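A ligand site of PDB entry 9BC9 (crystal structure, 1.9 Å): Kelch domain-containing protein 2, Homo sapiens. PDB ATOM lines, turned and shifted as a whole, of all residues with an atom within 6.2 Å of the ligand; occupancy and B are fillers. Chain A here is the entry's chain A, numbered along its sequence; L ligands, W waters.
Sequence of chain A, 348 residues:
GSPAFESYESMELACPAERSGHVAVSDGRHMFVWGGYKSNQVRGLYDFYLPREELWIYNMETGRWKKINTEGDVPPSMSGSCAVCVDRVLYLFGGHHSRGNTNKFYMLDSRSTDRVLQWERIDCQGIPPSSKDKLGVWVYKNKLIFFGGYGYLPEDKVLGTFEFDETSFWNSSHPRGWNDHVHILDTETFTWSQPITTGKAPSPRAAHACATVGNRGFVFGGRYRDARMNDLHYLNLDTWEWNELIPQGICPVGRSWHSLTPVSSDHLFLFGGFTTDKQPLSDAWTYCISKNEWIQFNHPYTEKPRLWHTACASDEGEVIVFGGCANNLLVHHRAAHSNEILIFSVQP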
ATOM      1  N   TYR A  37      -9.787  19.463  -3.338  1.00  0.00           N
ATOM      2  CA  TYR A  37     -10.922  19.380  -4.259  1.00  0.00           C
ATOM      3  C   TYR A  37     -11.677  18.084  -3.961  1.00  0.00           C
ATOM      4  O   TYR A  37     -11.198  17.214  -3.229  1.00  0.00           O
ATOM      5  CB  TYR A  37     -10.455  19.407  -5.721  1.00  0.00           C
ATOM      6  CG  TYR A  37      -9.959  18.052  -6.204  1.00  0.00           C
ATOM      7  CD1 TYR A  37      -8.784  17.504  -5.703  1.00  0.00           C
ATOM      8  CD2 TYR A  37     -10.683  17.314  -7.133  1.00  0.00           C
ATOM      9  CE1 TYR A  37      -8.327  16.261  -6.132  1.00  0.00           C
ATOM     10  CE2 TYR A  37     -10.237  16.072  -7.571  1.00  0.00           C
ATOM     11  CZ  TYR A  37      -9.057  15.544  -7.062  1.00  0.00           C
ATOM     12  OH  TYR A  37      -8.617  14.314  -7.489  1.00  0.00           O
ATOM     13  N   TYR A  49     -13.411  22.830  -6.319  1.00  0.00           N
ATOM     14  CA  TYR A  49     -12.524  23.119  -5.208  1.00  0.00           C
ATOM     15  C   TYR A  49     -13.336  23.455  -3.958  1.00  0.00           C
ATOM     16  O   TYR A  49     -14.447  23.985  -4.041  1.00  0.00           O
ATOM     17  CB  TYR A  49     -11.608  24.286  -5.571  1.00  0.00           C
ATOM     18  CG  TYR A  49     -10.650  24.000  -6.711  1.00  0.00           C
ATOM     19  CD1 TYR A  49      -9.561  23.165  -6.523  1.00  0.00           C
ATOM     20  CD2 TYR A  49     -10.832  24.570  -7.960  1.00  0.00           C
ATOM     21  CE1 TYR A  49      -8.678  22.898  -7.538  1.00  0.00           C
ATOM     22  CE2 TYR A  49      -9.954  24.306  -8.992  1.00  0.00           C
ATOM     23  CZ  TYR A  49      -8.878  23.473  -8.775  1.00  0.00           C
ATOM     24  OH  TYR A  49      -8.000  23.200  -9.796  1.00  0.00           O
ATOM     25  N   SER A  79      -5.555  22.865  -5.357  1.00  0.00           N
ATOM     26  CA  SER A  79      -5.067  21.517  -5.065  1.00  0.00           C
ATOM     27  C   SER A  79      -3.560  21.466  -5.301  1.00  0.00           C
ATOM     28  O   SER A  79      -3.031  22.175  -6.153  1.00  0.00           O
ATOM     29  CB  SER A  79      -5.769  20.475  -5.932  1.00  0.00           C
ATOM     30  OG  SER A  79      -5.314  20.559  -7.265  1.00  0.00           O
ATOM     31  N   HIS A  96      -2.628  24.467  -7.700  1.00  0.00           N
ATOM     32  CA  HIS A  96      -3.384  24.527  -8.951  1.00  0.00           C
ATOM     33  C   HIS A  96      -4.781  25.035  -8.647  1.00  0.00           C
ATOM     34  O   HIS A  96      -5.516  24.419  -7.861  1.00  0.00           O
ATOM     35  CB  HIS A  96      -3.452  23.153  -9.620  1.00  0.00           C
ATOM     36  CG  HIS A  96      -4.099  23.153 -10.965  1.00  0.00           C
ATOM     37  ND1 HIS A  96      -5.467  23.117 -11.136  1.00  0.00           N
ATOM     38  CD2 HIS A  96      -3.565  23.160 -12.212  1.00  0.00           C
ATOM     39  CE1 HIS A  96      -5.752  23.112 -12.431  1.00  0.00           C
ATOM     40  NE2 HIS A  96      -4.610  23.132 -13.103  1.00  0.00           N
ATOM     41  N   ASP A 133       2.867  22.662  -8.706  1.00  0.00           N
ATOM     42  CA  ASP A 133       2.154  22.035  -7.598  1.00  0.00           C
ATOM     43  C   ASP A 133       2.792  20.674  -7.295  1.00  0.00           C
ATOM     44  O   ASP A 133       3.735  20.246  -7.975  1.00  0.00           O
ATOM     45  CB  ASP A 133       0.661  21.907  -7.922  1.00  0.00           C
ATOM     46  CG  ASP A 133       0.379  21.006  -9.140  1.00  0.00           C
ATOM     47  OD1 ASP A 133       1.271  20.206  -9.532  1.00  0.00           O
ATOM     48  OD2 ASP A 133      -0.739  21.093  -9.708  1.00  0.00           O
ATOM     49  N   LYS A 134       2.252  19.981  -6.283  1.00  0.00           N
ATOM     50  CA  LYS A 134       2.653  18.609  -5.949  1.00  0.00           C
ATOM     51  C   LYS A 134       4.180  18.499  -5.784  1.00  0.00           C
ATOM     52  O   LYS A 134       4.838  17.648  -6.380  1.00  0.00           O
ATOM     53  CB  LYS A 134       2.134  17.582  -6.964  1.00  0.00           C
ATOM     54  CG  LYS A 134       0.636  17.736  -7.303  1.00  0.00           C
ATOM     55  CD  LYS A 134       0.082  16.486  -8.018  1.00  0.00           C
ATOM     56  CE  LYS A 134       0.492  16.432  -9.474  1.00  0.00           C
ATOM     57  NZ  LYS A 134      -0.021  17.608 -10.239  1.00  0.00           N
ATOM     58  N   TYR A 150       5.402  19.945 -10.422  1.00  0.00           N
ATOM     59  CA  TYR A 150       4.792  19.822 -11.749  1.00  0.00           C
ATOM     60  C   TYR A 150       4.097  21.128 -12.080  1.00  0.00           C
ATOM     61  O   TYR A 150       3.272  21.607 -11.300  1.00  0.00           O
ATOM     62  CB  TYR A 150       3.792  18.664 -11.756  1.00  0.00           C
ATOM     63  CG  TYR A 150       3.151  18.354 -13.091  1.00  0.00           C
ATOM     64  CD1 TYR A 150       3.821  17.623 -14.064  1.00  0.00           C
ATOM     65  CD2 TYR A 150       1.842  18.737 -13.355  1.00  0.00           C
ATOM     66  CE1 TYR A 150       3.216  17.300 -15.270  1.00  0.00           C
ATOM     67  CE2 TYR A 150       1.224  18.434 -14.555  1.00  0.00           C
ATOM     68  CZ  TYR A 150       1.917  17.715 -15.508  1.00  0.00           C
ATOM     69  OH  TYR A 150       1.305  17.419 -16.703  1.00  0.00           O
ATOM     70  N   ASP A 165       5.871  16.952 -19.890  1.00  0.00           N
ATOM     71  CA  ASP A 165       4.939  15.832 -19.901  1.00  0.00           C
ATOM     72  C   ASP A 165       4.217  15.843 -21.238  1.00  0.00           C
ATOM     73  O   ASP A 165       3.506  16.796 -21.558  1.00  0.00           O
ATOM     74  CB  ASP A 165       3.961  15.941 -18.733  1.00  0.00           C
ATOM     75  CG  ASP A 165       2.947  14.795 -18.684  1.00  0.00           C
ATOM     76  OD1 ASP A 165       3.032  13.859 -19.510  1.00  0.00           O
ATOM     77  OD2 ASP A 165       2.068  14.839 -17.797  1.00  0.00           O
ATOM     78  N   THR A 167       1.652  14.188 -22.499  1.00  0.00           N
ATOM     79  CA  THR A 167       0.197  14.155 -22.531  1.00  0.00           C
ATOM     80  C   THR A 167      -0.433  15.523 -22.316  1.00  0.00           C
ATOM     81  O   THR A 167      -1.589  15.731 -22.711  1.00  0.00           O
ATOM     82  CB  THR A 167      -0.327  13.171 -21.486  1.00  0.00           C
ATOM     83  OG1 THR A 167       0.294  13.435 -20.226  1.00  0.00           O
ATOM     84  CG2 THR A 167       0.006  11.743 -21.904  1.00  0.00           C
ATOM     85  N   ARG A 176       2.725  21.213 -19.443  1.00  0.00           N
ATOM     86  CA  ARG A 176       3.362  21.204 -18.134  1.00  0.00           C
ATOM     87  C   ARG A 176       4.393  20.082 -18.083  1.00  0.00           C
ATOM     88  O   ARG A 176       4.514  19.265 -19.011  1.00  0.00           O
ATOM     89  CB  ARG A 176       2.327  21.062 -17.018  1.00  0.00           C
ATOM     90  CG  ARG A 176       1.359  22.244 -16.945  1.00  0.00           C
ATOM     91  CD  ARG A 176       0.392  22.118 -15.787  1.00  0.00           C
ATOM     92  NE  ARG A 176      -0.711  21.209 -16.096  1.00  0.00           N
ATOM     93  CZ  ARG A 176      -1.604  20.788 -15.217  1.00  0.00           C
ATOM     94  NH1 ARG A 176      -1.528  21.143 -13.941  1.00  0.00           N
ATOM     95  NH2 ARG A 176      -2.590  19.997 -15.617  1.00  0.00           N
ATOM     96  N   TRP A 178       7.712  18.099 -15.232  1.00  0.00           N
ATOM     97  CA  TRP A 178       8.353  17.891 -13.931  1.00  0.00           C
ATOM     98  C   TRP A 178       9.708  18.570 -13.880  1.00  0.00           C
ATOM     99  O   TRP A 178      10.391  18.736 -14.892  1.00  0.00           O
ATOM    100  CB  TRP A 178       8.562  16.401 -13.652  1.00  0.00           C
ATOM    101  CG  TRP A 178       7.352  15.556 -13.763  1.00  0.00           C
ATOM    102  CD1 TRP A 178       6.464  15.238 -12.771  1.00  0.00           C
ATOM    103  CD2 TRP A 178       6.902  14.851 -14.933  1.00  0.00           C
ATOM    104  NE1 TRP A 178       5.481  14.418 -13.251  1.00  0.00           N
ATOM    105  CE2 TRP A 178       5.729  14.159 -14.578  1.00  0.00           C
ATOM    106  CE3 TRP A 178       7.372  14.767 -16.248  1.00  0.00           C
ATOM    107  CZ2 TRP A 178       5.017  13.382 -15.492  1.00  0.00           C
ATOM    108  CZ3 TRP A 178       6.665  13.998 -17.157  1.00  0.00           C
ATOM    109  CH2 TRP A 178       5.501  13.314 -16.766  1.00  0.00           C
ATOM    110  N   ARG A 205      10.613  15.355 -10.598  1.00  0.00           N
ATOM    111  CA  ARG A 205       9.511  14.535 -10.109  1.00  0.00           C
ATOM    112  C   ARG A 205       8.458  15.409  -9.456  1.00  0.00           C
ATOM    113  O   ARG A 205       8.705  16.572  -9.124  1.00  0.00           O
ATOM    114  CB  ARG A 205      10.008  13.464  -9.119  1.00  0.00           C
ATOM    115  CG  ARG A 205      10.770  14.010  -7.890  1.00  0.00           C
ATOM    116  CD  ARG A 205      11.461  12.866  -7.121  1.00  0.00           C
ATOM    117  NE  ARG A 205      12.493  12.222  -7.914  1.00  0.00           N
ATOM    118  CZ  ARG A 205      13.076  11.069  -7.615  1.00  0.00           C
ATOM    119  NH1 ARG A 205      12.719  10.351  -6.555  1.00  0.00           N
ATOM    120  NH2 ARG A 205      14.013  10.578  -8.438  1.00  0.00           N
ATOM    121  N   ALA A 206       7.272  14.828  -9.294  1.00  0.00           N
ATOM    122  CA  ALA A 206       6.207  15.438  -8.521  1.00  0.00           C
ATOM    123  C   ALA A 206       5.488  14.337  -7.751  1.00  0.00           C
ATOM    124  O   ALA A 206       5.644  13.151  -8.056  1.00  0.00           O
ATOM    125  CB  ALA A 206       5.216  16.207  -9.413  1.00  0.00           C
ATOM    126  N   ALA A 207       4.724  14.744  -6.744  1.00  0.00           N
ATOM    127  CA  ALA A 207       4.001  13.837  -5.850  1.00  0.00           C
ATOM    128  C   ALA A 207       4.948  12.935  -5.069  1.00  0.00           C
ATOM    129  O   ALA A 207       4.537  11.895  -4.534  1.00  0.00           O
ATOM    130  CB  ALA A 207       2.961  12.999  -6.621  1.00  0.00           C
ATOM    131  N   GLY A 222       7.979   9.363  -5.884  1.00  0.00           N
ATOM    132  CA  GLY A 222       7.522  10.377  -6.828  1.00  0.00           C
ATOM    133  C   GLY A 222       7.234   9.850  -8.224  1.00  0.00           C
ATOM    134  O   GLY A 222       7.686   8.770  -8.600  1.00  0.00           O
ATOM    135  N   ARG A 223       6.481  10.626  -8.994  1.00  0.00           N
ATOM    136  CA  ARG A 223       6.165  10.320 -10.382  1.00  0.00           C
ATOM    137  C   ARG A 223       7.141  11.024 -11.310  1.00  0.00           C
ATOM    138  O   ARG A 223       7.463  12.208 -11.095  1.00  0.00           O
ATOM    139  CB  ARG A 223       4.720  10.731 -10.709  1.00  0.00           C
ATOM    140  CG  ARG A 223       4.416  10.922 -12.199  1.00  0.00           C
ATOM    141  CD  ARG A 223       4.063   9.615 -12.884  1.00  0.00           C
ATOM    142  NE  ARG A 223       3.996   9.764 -14.340  1.00  0.00           N
ATOM    143  CZ  ARG A 223       2.960  10.277 -14.995  1.00  0.00           C
ATOM    144  NH1 ARG A 223       1.870  10.680 -14.357  1.00  0.00           N
ATOM    145  NH2 ARG A 223       3.038  10.407 -16.316  1.00  0.00           N
ATOM    146  N   TYR A 224       7.628  10.300 -12.309  1.00  0.00           N
ATOM    147  CA  TYR A 224       8.472  10.888 -13.336  1.00  0.00           C
ATOM    148  C   TYR A 224       8.369  10.033 -14.585  1.00  0.00           C
ATOM    149  O   TYR A 224       8.454   8.803 -14.507  1.00  0.00           O
ATOM    150  CB  TYR A 224       9.931  10.992 -12.877  1.00  0.00           C
ATOM    151  CG  TYR A 224      10.870  11.518 -13.943  1.00  0.00           C
ATOM    152  CD1 TYR A 224      12.013  10.805 -14.304  1.00  0.00           C
ATOM    153  CD2 TYR A 224      10.595  12.705 -14.611  1.00  0.00           C
ATOM    154  CE1 TYR A 224      12.863  11.271 -15.285  1.00  0.00           C
ATOM    155  CE2 TYR A 224      11.451  13.187 -15.597  1.00  0.00           C
ATOM    156  CZ  TYR A 224      12.582  12.462 -15.931  1.00  0.00           C
ATOM    157  OH  TYR A 224      13.420  12.933 -16.907  1.00  0.00           O
ATOM    158  N   ARG A 228       6.517   5.508 -11.229  1.00  0.00           N
ATOM    159  CA  ARG A 228       6.391   5.980  -9.870  1.00  0.00           C
ATOM    160  C   ARG A 228       7.460   5.268  -9.048  1.00  0.00           C
ATOM    161  O   ARG A 228       7.443   4.039  -8.908  1.00  0.00           O
ATOM    162  CB  ARG A 228       4.976   5.746  -9.335  1.00  0.00           C
ATOM    163  CG  ARG A 228       3.957   6.585 -10.133  1.00  0.00           C
ATOM    164  CD  ARG A 228       2.506   6.401  -9.731  1.00  0.00           C
ATOM    165  NE  ARG A 228       1.645   7.314 -10.482  1.00  0.00           N
ATOM    166  CZ  ARG A 228       0.918   6.976 -11.531  1.00  0.00           C
ATOM    167  NH1 ARG A 228       0.873   5.723 -11.979  1.00  0.00           N
ATOM    168  NH2 ARG A 228       0.208   7.909 -12.161  1.00  0.00           N
ATOM    169  N   SER A 256       3.824   7.272  -5.735  1.00  0.00           N
ATOM    170  CA  SER A 256       3.628   8.706  -5.591  1.00  0.00           C
ATOM    171  C   SER A 256       2.405   8.930  -4.719  1.00  0.00           C
ATOM    172  O   SER A 256       1.715   7.987  -4.331  1.00  0.00           O
ATOM    173  CB  SER A 256       3.455   9.382  -6.955  1.00  0.00           C
ATOM    174  OG  SER A 256       2.282   8.892  -7.597  1.00  0.00           O
ATOM    175  N   TRP A 257       2.143  10.197  -4.404  1.00  0.00           N
ATOM    176  CA  TRP A 257       0.944  10.606  -3.645  1.00  0.00           C
ATOM    177  C   TRP A 257       0.873   9.969  -2.247  1.00  0.00           C
ATOM    178  O   TRP A 257      -0.205   9.842  -1.660  1.00  0.00           O
ATOM    179  CB  TRP A 257      -0.331  10.319  -4.443  1.00  0.00           C
ATOM    180  CG  TRP A 257      -0.706  11.447  -5.327  1.00  0.00           C
ATOM    181  CD1 TRP A 257      -0.558  12.780  -5.040  1.00  0.00           C
ATOM    182  CD2 TRP A 257      -1.248  11.366  -6.644  1.00  0.00           C
ATOM    183  NE1 TRP A 257      -0.999  13.533  -6.097  1.00  0.00           N
ATOM    184  CE2 TRP A 257      -1.418  12.694  -7.102  1.00  0.00           C
ATOM    185  CE3 TRP A 257      -1.599  10.306  -7.473  1.00  0.00           C
ATOM    186  CZ2 TRP A 257      -1.946  12.982  -8.353  1.00  0.00           C
ATOM    187  CZ3 TRP A 257      -2.128  10.603  -8.734  1.00  0.00           C
ATOM    188  CH2 TRP A 257      -2.287  11.925  -9.160  1.00  0.00           C
ATOM    189  N   PHE A 274       0.391   5.399  -4.499  1.00  0.00           N
ATOM    190  CA  PHE A 274      -0.140   4.969  -5.784  1.00  0.00           C
ATOM    191  C   PHE A 274       1.012   4.405  -6.608  1.00  0.00           C
ATOM    192  O   PHE A 274       1.975   5.123  -6.892  1.00  0.00           O
ATOM    193  CB  PHE A 274      -0.783   6.175  -6.490  1.00  0.00           C
ATOM    194  CG  PHE A 274      -1.733   5.835  -7.609  1.00  0.00           C
ATOM    195  CD1 PHE A 274      -2.872   5.098  -7.363  1.00  0.00           C
ATOM    196  CD2 PHE A 274      -1.506   6.293  -8.895  1.00  0.00           C
ATOM    197  CE1 PHE A 274      -3.763   4.802  -8.390  1.00  0.00           C
ATOM    198  CE2 PHE A 274      -2.385   6.005  -9.923  1.00  0.00           C
ATOM    199  CZ  PHE A 274      -3.519   5.251  -9.664  1.00  0.00           C
ATOM    200  N   TRP A 308      -2.773  10.978  -2.029  1.00  0.00           N
ATOM    201  CA  TRP A 308      -2.981  12.432  -2.008  1.00  0.00           C
ATOM    202  C   TRP A 308      -3.710  12.859  -0.727  1.00  0.00           C
ATOM    203  O   TRP A 308      -4.418  13.876  -0.702  1.00  0.00           O
ATOM    204  CB  TRP A 308      -3.734  12.936  -3.251  1.00  0.00           C
ATOM    205  CG  TRP A 308      -3.220  14.258  -3.743  1.00  0.00           C
ATOM    206  CD1 TRP A 308      -2.216  14.994  -3.185  1.00  0.00           C
ATOM    207  CD2 TRP A 308      -3.669  14.983  -4.888  1.00  0.00           C
ATOM    208  NE1 TRP A 308      -2.008  16.141  -3.921  1.00  0.00           N
ATOM    209  CE2 TRP A 308      -2.891  16.158  -4.973  1.00  0.00           C
ATOM    210  CE3 TRP A 308      -4.662  14.767  -5.851  1.00  0.00           C
ATOM    211  CZ2 TRP A 308      -3.079  17.116  -5.974  1.00  0.00           C
ATOM    212  CZ3 TRP A 308      -4.837  15.705  -6.859  1.00  0.00           C
ATOM    213  CH2 TRP A 308      -4.055  16.874  -6.904  1.00  0.00           C
ATOM    214  N   LEU A 329      -7.902   8.203  -8.272  1.00  0.00           N
ATOM    215  CA  LEU A 329      -8.563   9.493  -8.414  1.00  0.00           C
ATOM    216  C   LEU A 329      -8.540  10.027  -9.844  1.00  0.00           C
ATOM    217  O   LEU A 329      -9.280  10.963 -10.152  1.00  0.00           O
ATOM    218  CB  LEU A 329      -7.938  10.525  -7.456  1.00  0.00           C
ATOM    219  CG  LEU A 329      -6.435  10.803  -7.467  1.00  0.00           C
ATOM    220  CD1 LEU A 329      -6.014  11.809  -8.526  1.00  0.00           C
ATOM    221  CD2 LEU A 329      -5.966  11.260  -6.098  1.00  0.00           C
ATOM    222  N   LEU A 330      -7.698   9.470 -10.715  1.00  0.00           N
ATOM    223  CA  LEU A 330      -7.709   9.898 -12.114  1.00  0.00           C
ATOM    224  C   LEU A 330      -8.967   9.488 -12.858  1.00  0.00           C
ATOM    225  O   LEU A 330      -9.181   9.969 -13.969  1.00  0.00           O
ATOM    226  CB  LEU A 330      -6.479   9.350 -12.850  1.00  0.00           C
ATOM    227  CG  LEU A 330      -5.131   9.668 -12.181  1.00  0.00           C
ATOM    228  CD1 LEU A 330      -3.999   8.836 -12.777  1.00  0.00           C
ATOM    229  CD2 LEU A 330      -4.821  11.155 -12.276  1.00  0.00           C
HETATM  230  N1  LIG L   1       1.099  13.481 -11.117  1.00  0.00           N
HETATM  231  C1  LIG L   1       1.453  12.515 -10.091  1.00  0.00           C
HETATM  232  C2  LIG L   1       1.241  11.082 -10.600  1.00  0.00           C
HETATM  233  O1  LIG L   1       0.929  10.852 -11.806  1.00  0.00           O
HETATM  234  O2  LIG L   1       1.391  10.114  -9.809  1.00  0.00           O
HETATM  235  C3  LIG L   1      -6.598  20.118 -10.272  1.00  0.00           C
HETATM  236  C4  LIG L   1      -6.537  17.842  -9.692  1.00  0.00           C
HETATM  237  C5  LIG L   1      -5.584  16.269 -11.115  1.00  0.00           C
HETATM  238  C6  LIG L   1      -5.132  16.975 -12.219  1.00  0.00           C
HETATM  239  C7  LIG L   1      -3.978  16.599 -12.879  1.00  0.00           C
HETATM  240  C8  LIG L   1      -3.263  15.488 -12.431  1.00  0.00           C
HETATM  241  C9  LIG L   1      -3.697  14.783 -11.327  1.00  0.00           C
HETATM  242  C10 LIG L   1      -4.863  15.165 -10.662  1.00  0.00           C
HETATM  243  C11 LIG L   1      -1.973  15.107 -13.166  1.00  0.00           C
HETATM  244  C12 LIG L   1       0.290  14.936 -13.466  1.00  0.00           C
HETATM  245  C13 LIG L   1       1.730  15.138 -12.991  1.00  0.00           C
HETATM  246  C14 LIG L   1       2.123  14.143 -11.914  1.00  0.00           C
HETATM  247  C15 LIG L   1      -0.061  14.359 -14.702  1.00  0.00           C
HETATM  248  N2  LIG L   1      -0.754  15.329 -12.679  1.00  0.00           N
HETATM  249  O3  LIG L   1      -7.324  18.935 -10.046  1.00  0.00           O
HETATM  250  O4  LIG L   1      -6.755  16.691 -10.473  1.00  0.00           O
HETATM  251  O5  LIG L   1       3.265  13.900 -11.740  1.00  0.00           O
HETATM  252  S1  LIG L   1      -1.761  14.398 -14.682  1.00  0.00           S
HETATM  253 CL1  LIG L   1      -3.421  17.524 -14.294  1.00  0.00          CL
HETATM  254  O   HOH W   1      -5.309  19.619 -14.763  1.00  0.00           O
HETATM  255  O   HOH W   2       1.119  12.008 -16.799  1.00  0.00           O
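Merely in contact with the ligand: Arg 176, Ser 79, His 96, Tyr 49, Tyr 150, Trp 257, Asp 165, Ala 206, Ala 207, Trp 308 and Leu 330.
Hydrophobic or aromatic side chains within 4 Å of the ligand: His 96, Tyr 150, Trp 178, Ala 206, Ala 207, Trp 257, Trp 308 and Leu 330.
Along chain A the residues within 4 Å of the ligand span positions 49 to 330.
NE1 of Trp 178 is in hydrogen-bond range of O5 of the ligand (2.7 Å).
The guanidinium group of Arg 223 lies within salt-bridge range of an oxygen (O1) of the ligand (2.7 Å).
OG of Ser 256 lies within hydrogen-bond range of O2 of the ligand (2.7 Å).
The guanidinium group of Arg 228 is in salt-bridge range of an oxygen (O2) of the ligand.
A nitrogen (N2) of the ligand is in hydrogen-bond range of the side-chain amino group (NZ) of Lys 134.
Water W2 bridges NH2 of Arg 223 (2.5 Å) and OD2 of Asp 165 (3.1 Å).
The backbone NH of Ala 207 is in hydrogen-bond range of the backbone carbonyl oxygen of Lys 134 (2.9 Å).
O of Ala 206 is in hydrogen-bond range of N of Arg 223, 2.8 Å away.
O of Trp 257 lies within hydrogen-bond range of N of Trp 308 (2.8 Å).
The side-chain amino group (NZ) of Lys 134 lies within salt-bridge range of the side-chain carboxylate (OD1) of Asp 133 (3.0 Å).
The backbone NH (N) of Trp 257 lies within hydrogen-bond range of the backbone carbonyl oxygen (O) of Ala 207, 2.9 Å away.
OD2 of Asp 165 is in hydrogen-bond range of OH of Tyr 150, at 2.9 Å.
The side-chain carboxylate (OD1) of Asp 165 is in hydrogen-bond range of the side-chain hydroxyl (OG1) of Thr 167 (2.9 Å).
OG of Ser 256 lies close to NE of Arg 228 (3.3 Å).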
